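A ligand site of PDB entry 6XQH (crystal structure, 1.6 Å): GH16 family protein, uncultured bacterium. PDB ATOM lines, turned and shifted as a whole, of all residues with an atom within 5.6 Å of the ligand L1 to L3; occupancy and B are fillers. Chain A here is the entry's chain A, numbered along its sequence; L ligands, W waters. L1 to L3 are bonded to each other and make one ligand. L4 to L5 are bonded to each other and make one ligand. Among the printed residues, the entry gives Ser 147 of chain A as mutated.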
ATOM      1  N   TYR A  55       7.382   5.561   1.027  1.00  0.00           N
ATOM      2  CA  TYR A  55       6.965   4.172   1.192  1.00  0.00           C
ATOM      3  C   TYR A  55       6.644   3.537  -0.169  1.00  0.00           C
ATOM      4  O   TYR A  55       6.691   4.210  -1.217  1.00  0.00           O
ATOM      5  CB  TYR A  55       5.841   4.119   2.230  1.00  0.00           C
ATOM      6  CG  TYR A  55       6.215   4.716   3.558  1.00  0.00           C
ATOM      7  CD1 TYR A  55       7.030   4.035   4.458  1.00  0.00           C
ATOM      8  CD2 TYR A  55       5.725   5.967   3.918  1.00  0.00           C
ATOM      9  CE1 TYR A  55       7.397   4.598   5.671  1.00  0.00           C
ATOM     10  CE2 TYR A  55       6.015   6.515   5.150  1.00  0.00           C
ATOM     11  CZ  TYR A  55       6.826   5.830   6.026  1.00  0.00           C
ATOM     12  OH  TYR A  55       7.247   6.350   7.227  1.00  0.00           O
ATOM     13  N   ASN A  56       6.316   2.240  -0.123  1.00  0.00           N
ATOM     14  CA  ASN A  56       5.882   1.492  -1.333  1.00  0.00           C
ATOM     15  C   ASN A  56       6.977   1.483  -2.387  1.00  0.00           C
ATOM     16  O   ASN A  56       6.642   1.357  -3.559  1.00  0.00           O
ATOM     17  CB  ASN A  56       4.596   2.091  -1.891  1.00  0.00           C
ATOM     18  CG  ASN A  56       3.515   2.185  -0.846  1.00  0.00           C
ATOM     19  OD1 ASN A  56       3.250   1.151  -0.194  1.00  0.00           O
ATOM     20  ND2 ASN A  56       2.933   3.370  -0.675  1.00  0.00           N
ATOM     21  N   GLU A  58       8.495   3.898  -3.519  1.00  0.00           N
ATOM     22  CA  GLU A  58       8.162   4.978  -4.484  1.00  0.00           C
ATOM     23  C   GLU A  58       9.425   5.759  -4.886  1.00  0.00           C
ATOM     24  O   GLU A  58      10.441   5.791  -4.126  1.00  0.00           O
ATOM     25  CB  GLU A  58       7.156   5.903  -3.850  1.00  0.00           C
ATOM     26  CG  GLU A  58       5.758   5.300  -3.850  1.00  0.00           C
ATOM     27  CD  GLU A  58       4.802   5.950  -2.858  1.00  0.00           C
ATOM     28  OE1 GLU A  58       5.065   7.074  -2.396  1.00  0.00           O
ATOM     29  OE2 GLU A  58       3.751   5.306  -2.605  1.00  0.00           O
ATOM     30  N   LYS A 101       2.165  16.196  -3.262  1.00  0.00           N
ATOM     31  CA  LYS A 101       1.257  15.527  -2.307  1.00  0.00           C
ATOM     32  C   LYS A 101       0.734  16.592  -1.358  1.00  0.00           C
ATOM     33  O   LYS A 101       1.552  17.217  -0.673  1.00  0.00           O
ATOM     34  CB  LYS A 101       1.967  14.464  -1.490  1.00  0.00           C
ATOM     35  CG  LYS A 101       1.110  13.907  -0.362  1.00  0.00           C
ATOM     36  CD  LYS A 101       1.757  12.683   0.275  1.00  0.00           C
ATOM     37  CE  LYS A 101       0.895  12.192   1.415  1.00  0.00           C
ATOM     38  NZ  LYS A 101       1.568  11.161   2.218  1.00  0.00           N
ATOM     39  N   TRP A 128       1.048   6.865 -10.456  1.00  0.00           N
ATOM     40  CA  TRP A 128       0.171   6.303  -9.403  1.00  0.00           C
ATOM     41  C   TRP A 128      -0.560   7.450  -8.752  1.00  0.00           C
ATOM     42  O   TRP A 128      -0.318   7.828  -7.607  1.00  0.00           O
ATOM     43  CB  TRP A 128       1.019   5.528  -8.417  1.00  0.00           C
ATOM     44  CG  TRP A 128       0.250   4.798  -7.381  1.00  0.00           C
ATOM     45  CD1 TRP A 128      -1.094   4.746  -7.125  1.00  0.00           C
ATOM     46  CD2 TRP A 128       0.894   4.105  -6.318  1.00  0.00           C
ATOM     47  NE1 TRP A 128      -1.304   4.007  -5.979  1.00  0.00           N
ATOM     48  CE2 TRP A 128      -0.089   3.598  -5.464  1.00  0.00           C
ATOM     49  CE3 TRP A 128       2.238   3.828  -6.054  1.00  0.00           C
ATOM     50  CZ2 TRP A 128       0.240   2.841  -4.349  1.00  0.00           C
ATOM     51  CZ3 TRP A 128       2.564   3.046  -4.965  1.00  0.00           C
ATOM     52  CH2 TRP A 128       1.569   2.565  -4.104  1.00  0.00           C
ATOM     53  N   ALA A 130      -3.596   9.227  -6.798  1.00  0.00           N
ATOM     54  CA  ALA A 130      -4.401   8.755  -5.652  1.00  0.00           C
ATOM     55  C   ALA A 130      -5.168   9.922  -5.060  1.00  0.00           C
ATOM     56  O   ALA A 130      -4.667  11.030  -4.985  1.00  0.00           O
ATOM     57  CB  ALA A 130      -3.570   8.083  -4.602  1.00  0.00           C
ATOM     58  N   TRP A 132      -7.254   9.950  -1.506  1.00  0.00           N
ATOM     59  CA  TRP A 132      -7.458   9.033  -0.379  1.00  0.00           C
ATOM     60  C   TRP A 132      -7.506   9.815   0.923  1.00  0.00           C
ATOM     61  O   TRP A 132      -7.295  10.991   0.936  1.00  0.00           O
ATOM     62  CB  TRP A 132      -6.371   7.959  -0.414  1.00  0.00           C
ATOM     63  CG  TRP A 132      -4.923   8.359  -0.370  1.00  0.00           C
ATOM     64  CD1 TRP A 132      -4.242   9.180  -1.221  1.00  0.00           C
ATOM     65  CD2 TRP A 132      -3.964   7.969   0.635  1.00  0.00           C
ATOM     66  NE1 TRP A 132      -2.930   9.268  -0.829  1.00  0.00           N
ATOM     67  CE2 TRP A 132      -2.732   8.561   0.317  1.00  0.00           C
ATOM     68  CE3 TRP A 132      -4.015   7.200   1.796  1.00  0.00           C
ATOM     69  CZ2 TRP A 132      -1.561   8.311   1.031  1.00  0.00           C
ATOM     70  CZ3 TRP A 132      -2.873   6.993   2.522  1.00  0.00           C
ATOM     71  CH2 TRP A 132      -1.665   7.574   2.159  1.00  0.00           C
ATOM     72  N   MET A 134      -6.770   9.383   5.366  1.00  0.00           N
ATOM     73  CA  MET A 134      -6.242   8.717   6.565  1.00  0.00           C
ATOM     74  C   MET A 134      -6.852   9.376   7.791  1.00  0.00           C
ATOM     75  O   MET A 134      -7.232  10.508   7.732  1.00  0.00           O
ATOM     76  CB  MET A 134      -4.724   8.806   6.643  1.00  0.00           C
ATOM     77  CG  MET A 134      -3.998   7.859   5.716  1.00  0.00           C
ATOM     78  SD  MET A 134      -2.197   8.160   5.661  1.00  0.00           S
ATOM     79  CE  MET A 134      -1.796   7.388   7.225  1.00  0.00           C
ATOM     80  N   TRP A 142      -0.159   3.327  11.117  1.00  0.00           N
ATOM     81  CA  TRP A 142      -0.590   2.689   9.871  1.00  0.00           C
ATOM     82  C   TRP A 142      -0.190   1.243   9.931  1.00  0.00           C
ATOM     83  O   TRP A 142       0.947   0.929  10.262  1.00  0.00           O
ATOM     84  CB  TRP A 142       0.030   3.365   8.654  1.00  0.00           C
ATOM     85  CG  TRP A 142      -0.673   2.952   7.396  1.00  0.00           C
ATOM     86  CD1 TRP A 142      -1.734   3.531   6.830  1.00  0.00           C
ATOM     87  CD2 TRP A 142      -0.435   1.727   6.682  1.00  0.00           C
ATOM     88  NE1 TRP A 142      -2.202   2.770   5.768  1.00  0.00           N
ATOM     89  CE2 TRP A 142      -1.401   1.661   5.668  1.00  0.00           C
ATOM     90  CE3 TRP A 142       0.511   0.705   6.817  1.00  0.00           C
ATOM     91  CZ2 TRP A 142      -1.453   0.590   4.775  1.00  0.00           C
ATOM     92  CZ3 TRP A 142       0.487  -0.337   5.895  1.00  0.00           C
ATOM     93  CH2 TRP A 142      -0.480  -0.359   4.884  1.00  0.00           C
ATOM     94  N   SER A 147      -7.472   3.805   6.597  1.00  0.00           N
ATOM     95  CA  SER A 147      -7.177   4.585   5.360  1.00  0.00           C
ATOM     96  C   SER A 147      -8.258   4.286   4.312  1.00  0.00           C
ATOM     97  O   SER A 147      -8.710   3.131   4.289  1.00  0.00           O
ATOM     98  CB  SER A 147      -5.818   4.258   4.768  1.00  0.00           C
ATOM     99  OG  SER A 147      -4.786   4.201   5.750  1.00  0.00           O
ATOM    100  N   ASP A 149      -8.984   4.666   0.267  1.00  0.00           N
ATOM    101  CA  ASP A 149      -8.556   5.024  -1.090  1.00  0.00           C
ATOM    102  C   ASP A 149      -9.786   5.206  -1.956  1.00  0.00           C
ATOM    103  O   ASP A 149     -10.295   4.239  -2.466  1.00  0.00           O
ATOM    104  CB  ASP A 149      -7.594   3.976  -1.609  1.00  0.00           C
ATOM    105  CG  ASP A 149      -6.251   4.016  -0.920  1.00  0.00           C
ATOM    106  OD1 ASP A 149      -5.412   4.842  -1.413  1.00  0.00           O
ATOM    107  OD2 ASP A 149      -6.045   3.154  -0.055  1.00  0.00           O
ATOM    108  N   GLU A 152      -7.457   5.038  -6.628  1.00  0.00           N
ATOM    109  CA  GLU A 152      -6.080   4.866  -7.114  1.00  0.00           C
ATOM    110  C   GLU A 152      -6.149   4.380  -8.528  1.00  0.00           C
ATOM    111  O   GLU A 152      -7.020   3.565  -8.874  1.00  0.00           O
ATOM    112  CB  GLU A 152      -5.335   3.863  -6.243  1.00  0.00           C
ATOM    113  CG  GLU A 152      -5.079   4.412  -4.873  1.00  0.00           C
ATOM    114  CD  GLU A 152      -4.541   3.346  -3.968  1.00  0.00           C
ATOM    115  OE1 GLU A 152      -5.359   2.515  -3.445  1.00  0.00           O
ATOM    116  OE2 GLU A 152      -3.261   3.205  -3.892  1.00  0.00           O
ATOM    117  N   HIS A 166      -8.149   0.147   4.097  1.00  0.00           N
ATOM    118  CA  HIS A 166      -7.108  -0.556   4.867  1.00  0.00           C
ATOM    119  C   HIS A 166      -7.379  -0.328   6.342  1.00  0.00           C
ATOM    120  O   HIS A 166      -7.721   0.807   6.718  1.00  0.00           O
ATOM    121  CB  HIS A 166      -5.719  -0.081   4.515  1.00  0.00           C
ATOM    122  CG  HIS A 166      -5.408  -0.184   3.055  1.00  0.00           C
ATOM    123  ND1 HIS A 166      -4.743  -1.275   2.519  1.00  0.00           N
ATOM    124  CD2 HIS A 166      -5.665   0.672   2.045  1.00  0.00           C
ATOM    125  CE1 HIS A 166      -4.628  -1.084   1.220  1.00  0.00           C
ATOM    126  NE2 HIS A 166      -5.171   0.138   0.883  1.00  0.00           N
ATOM    127  N   HIS A 172      -2.920  -4.144   2.786  1.00  0.00           N
ATOM    128  CA  HIS A 172      -2.172  -4.744   1.659  1.00  0.00           C
ATOM    129  C   HIS A 172      -0.938  -5.469   2.141  1.00  0.00           C
ATOM    130  O   HIS A 172      -0.470  -6.400   1.417  1.00  0.00           O
ATOM    131  CB  HIS A 172      -1.835  -3.744   0.586  1.00  0.00           C
ATOM    132  CG  HIS A 172      -0.873  -2.667   0.978  1.00  0.00           C
ATOM    133  ND1 HIS A 172       0.500  -2.872   1.006  1.00  0.00           N
ATOM    134  CD2 HIS A 172      -1.086  -1.387   1.356  1.00  0.00           C
ATOM    135  CE1 HIS A 172       1.077  -1.716   1.372  1.00  0.00           C
ATOM    136  NE2 HIS A 172       0.143  -0.797   1.565  1.00  0.00           N
ATOM    137  N   VAL A 173      -0.417  -5.158   3.321  1.00  0.00           N
ATOM    138  CA  VAL A 173       0.894  -5.747   3.714  1.00  0.00           C
ATOM    139  C   VAL A 173       0.702  -7.234   3.910  1.00  0.00           C
ATOM    140  O   VAL A 173       1.578  -8.039   3.598  1.00  0.00           O
ATOM    141  CB  VAL A 173       1.435  -5.064   4.991  1.00  0.00           C
ATOM    142  CG1 VAL A 173       2.624  -5.826   5.561  1.00  0.00           C
ATOM    143  CG2 VAL A 173       1.751  -3.625   4.728  1.00  0.00           C
ATOM    144  N   ASN A 237      -2.358  13.042  -4.353  1.00  0.00           N
ATOM    145  CA  ASN A 237      -0.950  12.977  -4.741  1.00  0.00           C
ATOM    146  C   ASN A 237      -0.817  12.250  -6.056  1.00  0.00           C
ATOM    147  O   ASN A 237      -1.746  11.557  -6.509  1.00  0.00           O
ATOM    148  CB  ASN A 237      -0.123  12.229  -3.696  1.00  0.00           C
ATOM    149  CG  ASN A 237      -0.557  10.796  -3.552  1.00  0.00           C
ATOM    150  OD1 ASN A 237      -1.586  10.541  -2.891  1.00  0.00           O
ATOM    151  ND2 ASN A 237       0.192   9.869  -4.127  1.00  0.00           N
HETATM  152  C1  LIG L   1      -2.996   3.092   0.093  1.00  0.00           C
HETATM  153  C2  LIG L   1      -1.633   2.623   0.584  1.00  0.00           C
HETATM  154  C3  LIG L   1      -0.659   3.765   0.799  1.00  0.00           C
HETATM  155  C4  LIG L   1      -0.608   4.518  -0.474  1.00  0.00           C
HETATM  156  C5  LIG L   1      -2.001   5.099  -0.740  1.00  0.00           C
HETATM  157  C6  LIG L   1      -2.072   6.068  -1.901  1.00  0.00           C
HETATM  158  O1  LIG L   1      -3.632   3.611   1.255  1.00  0.00           O
HETATM  159  O2  LIG L   1      -1.871   1.764   1.721  1.00  0.00           O
HETATM  160  O3  LIG L   1       0.634   3.263   1.146  1.00  0.00           O
HETATM  161  O4  LIG L   1       0.334   5.619  -0.265  1.00  0.00           O
HETATM  162  O5  LIG L   1      -2.890   4.035  -0.967  1.00  0.00           O
HETATM  163  O6  LIG L   1      -1.751   5.330  -3.065  1.00  0.00           O
HETATM  164  C1  LG2 L   2       2.191   2.474   2.695  1.00  0.00           C
HETATM  165  C2  LG2 L   2       2.536   2.343   4.141  1.00  0.00           C
HETATM  166  C3  LG2 L   2       2.471   3.772   4.771  1.00  0.00           C
HETATM  167  C4  LG2 L   2       1.176   4.407   4.431  1.00  0.00           C
HETATM  168  C5  LG2 L   2       1.006   5.821   4.914  1.00  0.00           C
HETATM  169  C6  LG2 L   2       0.849   3.145   2.512  1.00  0.00           C
HETATM  170  O1  LG2 L   2       2.090   1.127   2.160  1.00  0.00           O
HETATM  171  O2  LG2 L   2       3.856   1.789   4.299  1.00  0.00           O
HETATM  172  O3  LG2 L   2       2.565   3.794   6.234  1.00  0.00           O
HETATM  173  O4  LG2 L   2       0.946   4.432   3.064  1.00  0.00           O
HETATM  174  O5  LG2 L   2       2.013   6.570   4.295  1.00  0.00           O
HETATM  175  C1  LG3 L   3       3.696   4.335   8.155  1.00  0.00           C
HETATM  176  C2  LG3 L   3       4.912   4.001   9.027  1.00  0.00           C
HETATM  177  C3  LG3 L   3       5.190   2.520   9.040  1.00  0.00           C
HETATM  178  C4  LG3 L   3       5.277   1.948   7.604  1.00  0.00           C
HETATM  179  C5  LG3 L   3       5.364   0.446   7.639  1.00  0.00           C
HETATM  180  C6  LG3 L   3       3.813   3.632   6.823  1.00  0.00           C
HETATM  181  O1  LG3 L   3       3.514   5.742   7.960  1.00  0.00           O
HETATM  182  O2  LG3 L   3       4.760   4.501  10.374  1.00  0.00           O
HETATM  183  O3  LG3 L   3       6.394   2.233   9.712  1.00  0.00           O
HETATM  184  O4  LG3 L   3       4.065   2.271   6.942  1.00  0.00           O
HETATM  185  O5  LG3 L   3       5.650  -0.012   6.289  1.00  0.00           O
HETATM  186  C1  LG4 L   4      -4.823  -5.413  -5.997  1.00  0.00           C
HETATM  187  C2  LG4 L   4      -4.828  -4.336  -4.987  1.00  0.00           C
HETATM  188  C3  LG4 L   4      -3.734  -4.737  -3.999  1.00  0.00           C
HETATM  189  C4  LG4 L   4      -2.349  -4.932  -4.625  1.00  0.00           C
HETATM  190  C5  LG4 L   4      -1.176  -5.139  -3.654  1.00  0.00           C
HETATM  191  C6  LG4 L   4      -3.380  -5.668  -6.490  1.00  0.00           C
HETATM  192  O1  LG4 L   4      -3.343  -6.682  -7.493  1.00  0.00           O
HETATM  193  O2  LG4 L   4      -5.733  -4.911  -6.995  1.00  0.00           O
HETATM  194  O3  LG4 L   4      -6.160  -4.201  -4.395  1.00  0.00           O
HETATM  195  O4  LG4 L   4      -3.796  -3.740  -3.020  1.00  0.00           O
HETATM  196  O5  LG4 L   4      -2.581  -6.115  -5.385  1.00  0.00           O
HETATM  197  O6  LG4 L   4      -1.515  -6.222  -2.775  1.00  0.00           O
HETATM  198  C1  LG5 L   5      -4.418  -1.622  -2.644  1.00  0.00           C
HETATM  199  C2  LG5 L   5      -4.014  -0.143  -2.656  1.00  0.00           C
HETATM  200  C3  LG5 L   5      -2.552  -0.026  -2.206  1.00  0.00           C
HETATM  201  C4  LG5 L   5      -1.579  -0.935  -2.887  1.00  0.00           C
HETATM  202  C5  LG5 L   5      -0.228  -0.830  -2.245  1.00  0.00           C
HETATM  203  C6  LG5 L   5      -3.344  -2.432  -3.317  1.00  0.00           C
HETATM  204  O1  LG5 L   5      -5.678  -1.772  -3.357  1.00  0.00           O
HETATM  205  O2  LG5 L   5      -4.973   0.574  -1.915  1.00  0.00           O
HETATM  206  O3  LG5 L   5      -2.117   1.304  -2.345  1.00  0.00           O
HETATM  207  O4  LG5 L   5      -2.068  -2.236  -2.638  1.00  0.00           O
HETATM  208  O5  LG5 L   5       0.712  -1.609  -3.022  1.00  0.00           O
HETATM  209  O   HOH W   1       2.727   3.840  11.754  1.00  0.00           O
HETATM  210  O   HOH W   2       1.345   6.477  -2.580  1.00  0.00           O
HETATM  211  O   HOH W   3       2.232   6.590   1.503  1.00  0.00           O
HETATM  212  O   HOH W   4       4.291  -0.799   3.249  1.00  0.00           O
HETATM  213  O   HOH W   5       2.119   9.095   5.861  1.00  0.00           O
HETATM  214  O   HOH W   6       5.933   0.656   2.257  1.00  0.00           O
HETATM  215  O   HOH W   7       1.260   6.961   8.442  1.00  0.00           O
HETATM  216  O   HOH W   8      -0.250   6.985  -4.790  1.00  0.00           O
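Water W1 lies within hydrogen-bond range of O2 of LG3 L3 (2.5 Å) and N of Trp 142 (3.0 Å). Water W2 bridges O4 of LIG L1 and OE2 of Glu 58. Water W8 lies within hydrogen-bond range of an oxygen (O6) of LIG L1 (2.8 Å), the backbone carbonyl oxygen (O) of Trp 128 (2.9 Å) and the side-chain amide nitrogen (ND2) of Asn 237 (3.0 Å). Water W6 lies within hydrogen-bond range of N of Asn 56 (2.9 Å) and O2 of LG2 L2 (3.1 Å).
O1 of LG2 L2 sits at hydrogen-bond distance from OD1 of Asn 56 (2.6 Å). The side-chain carboxylate (OD2) of Asp 149 sits at hydrogen-bond distance from an oxygen (O1) of LIG L1. O6 of LIG L1 lies within hydrogen-bond range of OE2 of Glu 152 (2.7 Å). NE2 of His 172 lies within hydrogen-bond range of O1 of LG2 L2 (2.8 Å). The indole nitrogen of Trp 128 is in hydrogen-bond range of an oxygen (O6) of LIG L1, at 3.2 Å. An oxygen (O2) of LG5 L5 is in hydrogen-bond range of the side-chain carboxylate (OD2) of Asp 149 (3.4 Å). The side-chain carboxylate of Glu 152 lies within hydrogen-bond range of an oxygen (O2) of LG5 L5 (2.5 Å). A ring nitrogen (NE2) of His 166 is in hydrogen-bond range of an oxygen (O2) of LG5 L5 (2.8 Å).
ND2 of Asn 56 sits at hydrogen-bond distance from OE2 of Glu 58. OD2 of Asp 149 sits close to NE2 of His 166 (3.3 Å). The indole nitrogen (NE1) of Trp 128 is in hydrogen-bond range of the side-chain carboxylate (OE2) of Glu 152, at 3.0 Å. ND1 of His 166 sits at hydrogen-bond distance from N of His 172, at 3.4 Å. NE1 of Trp 142 is in hydrogen-bond range of OG of Ser 147, at 3.0 Å. The indole nitrogen (NE1) of Trp 132 is in hydrogen-bond range of the side-chain amide oxygen (OD1) of Asn 237 (2.8 Å). The backbone NH of Ala 130 sits at hydrogen-bond distance from the backbone carbonyl oxygen of Asn 237 (3.0 Å). O of His 166 lies within hydrogen-bond range of N of Ser 147.
O5 of LIG L1 sits close to O3 of LG5 L5.
Tyr 55 touches the ligand L1 to L3. Ala 130 touches the ligand L1 to L3. CE2 of Trp 132 touches C6 of LIG L1, at 3.4 Å. Met 134 touches the ligand L1 to L3. CZ2 of Trp 142 touches O2 of LIG L1, at 3.3 Å. CD2 of His 166 touches O1 of LIG L1, 3.7 Å away. Hydrophobic or aromatic side chains within 4 Å of the ligand L1 to L3: Tyr 55, Trp 128, Ala 130, Trp 132, Met 134, Trp 142, His 166 and His 172. Of the 16 residues printed, 11 come within 4 Å of the ligand L1 to L3. The nearest printed residue that does not touch the ligand L1 to L3 is Glu 58 (4.2 Å).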
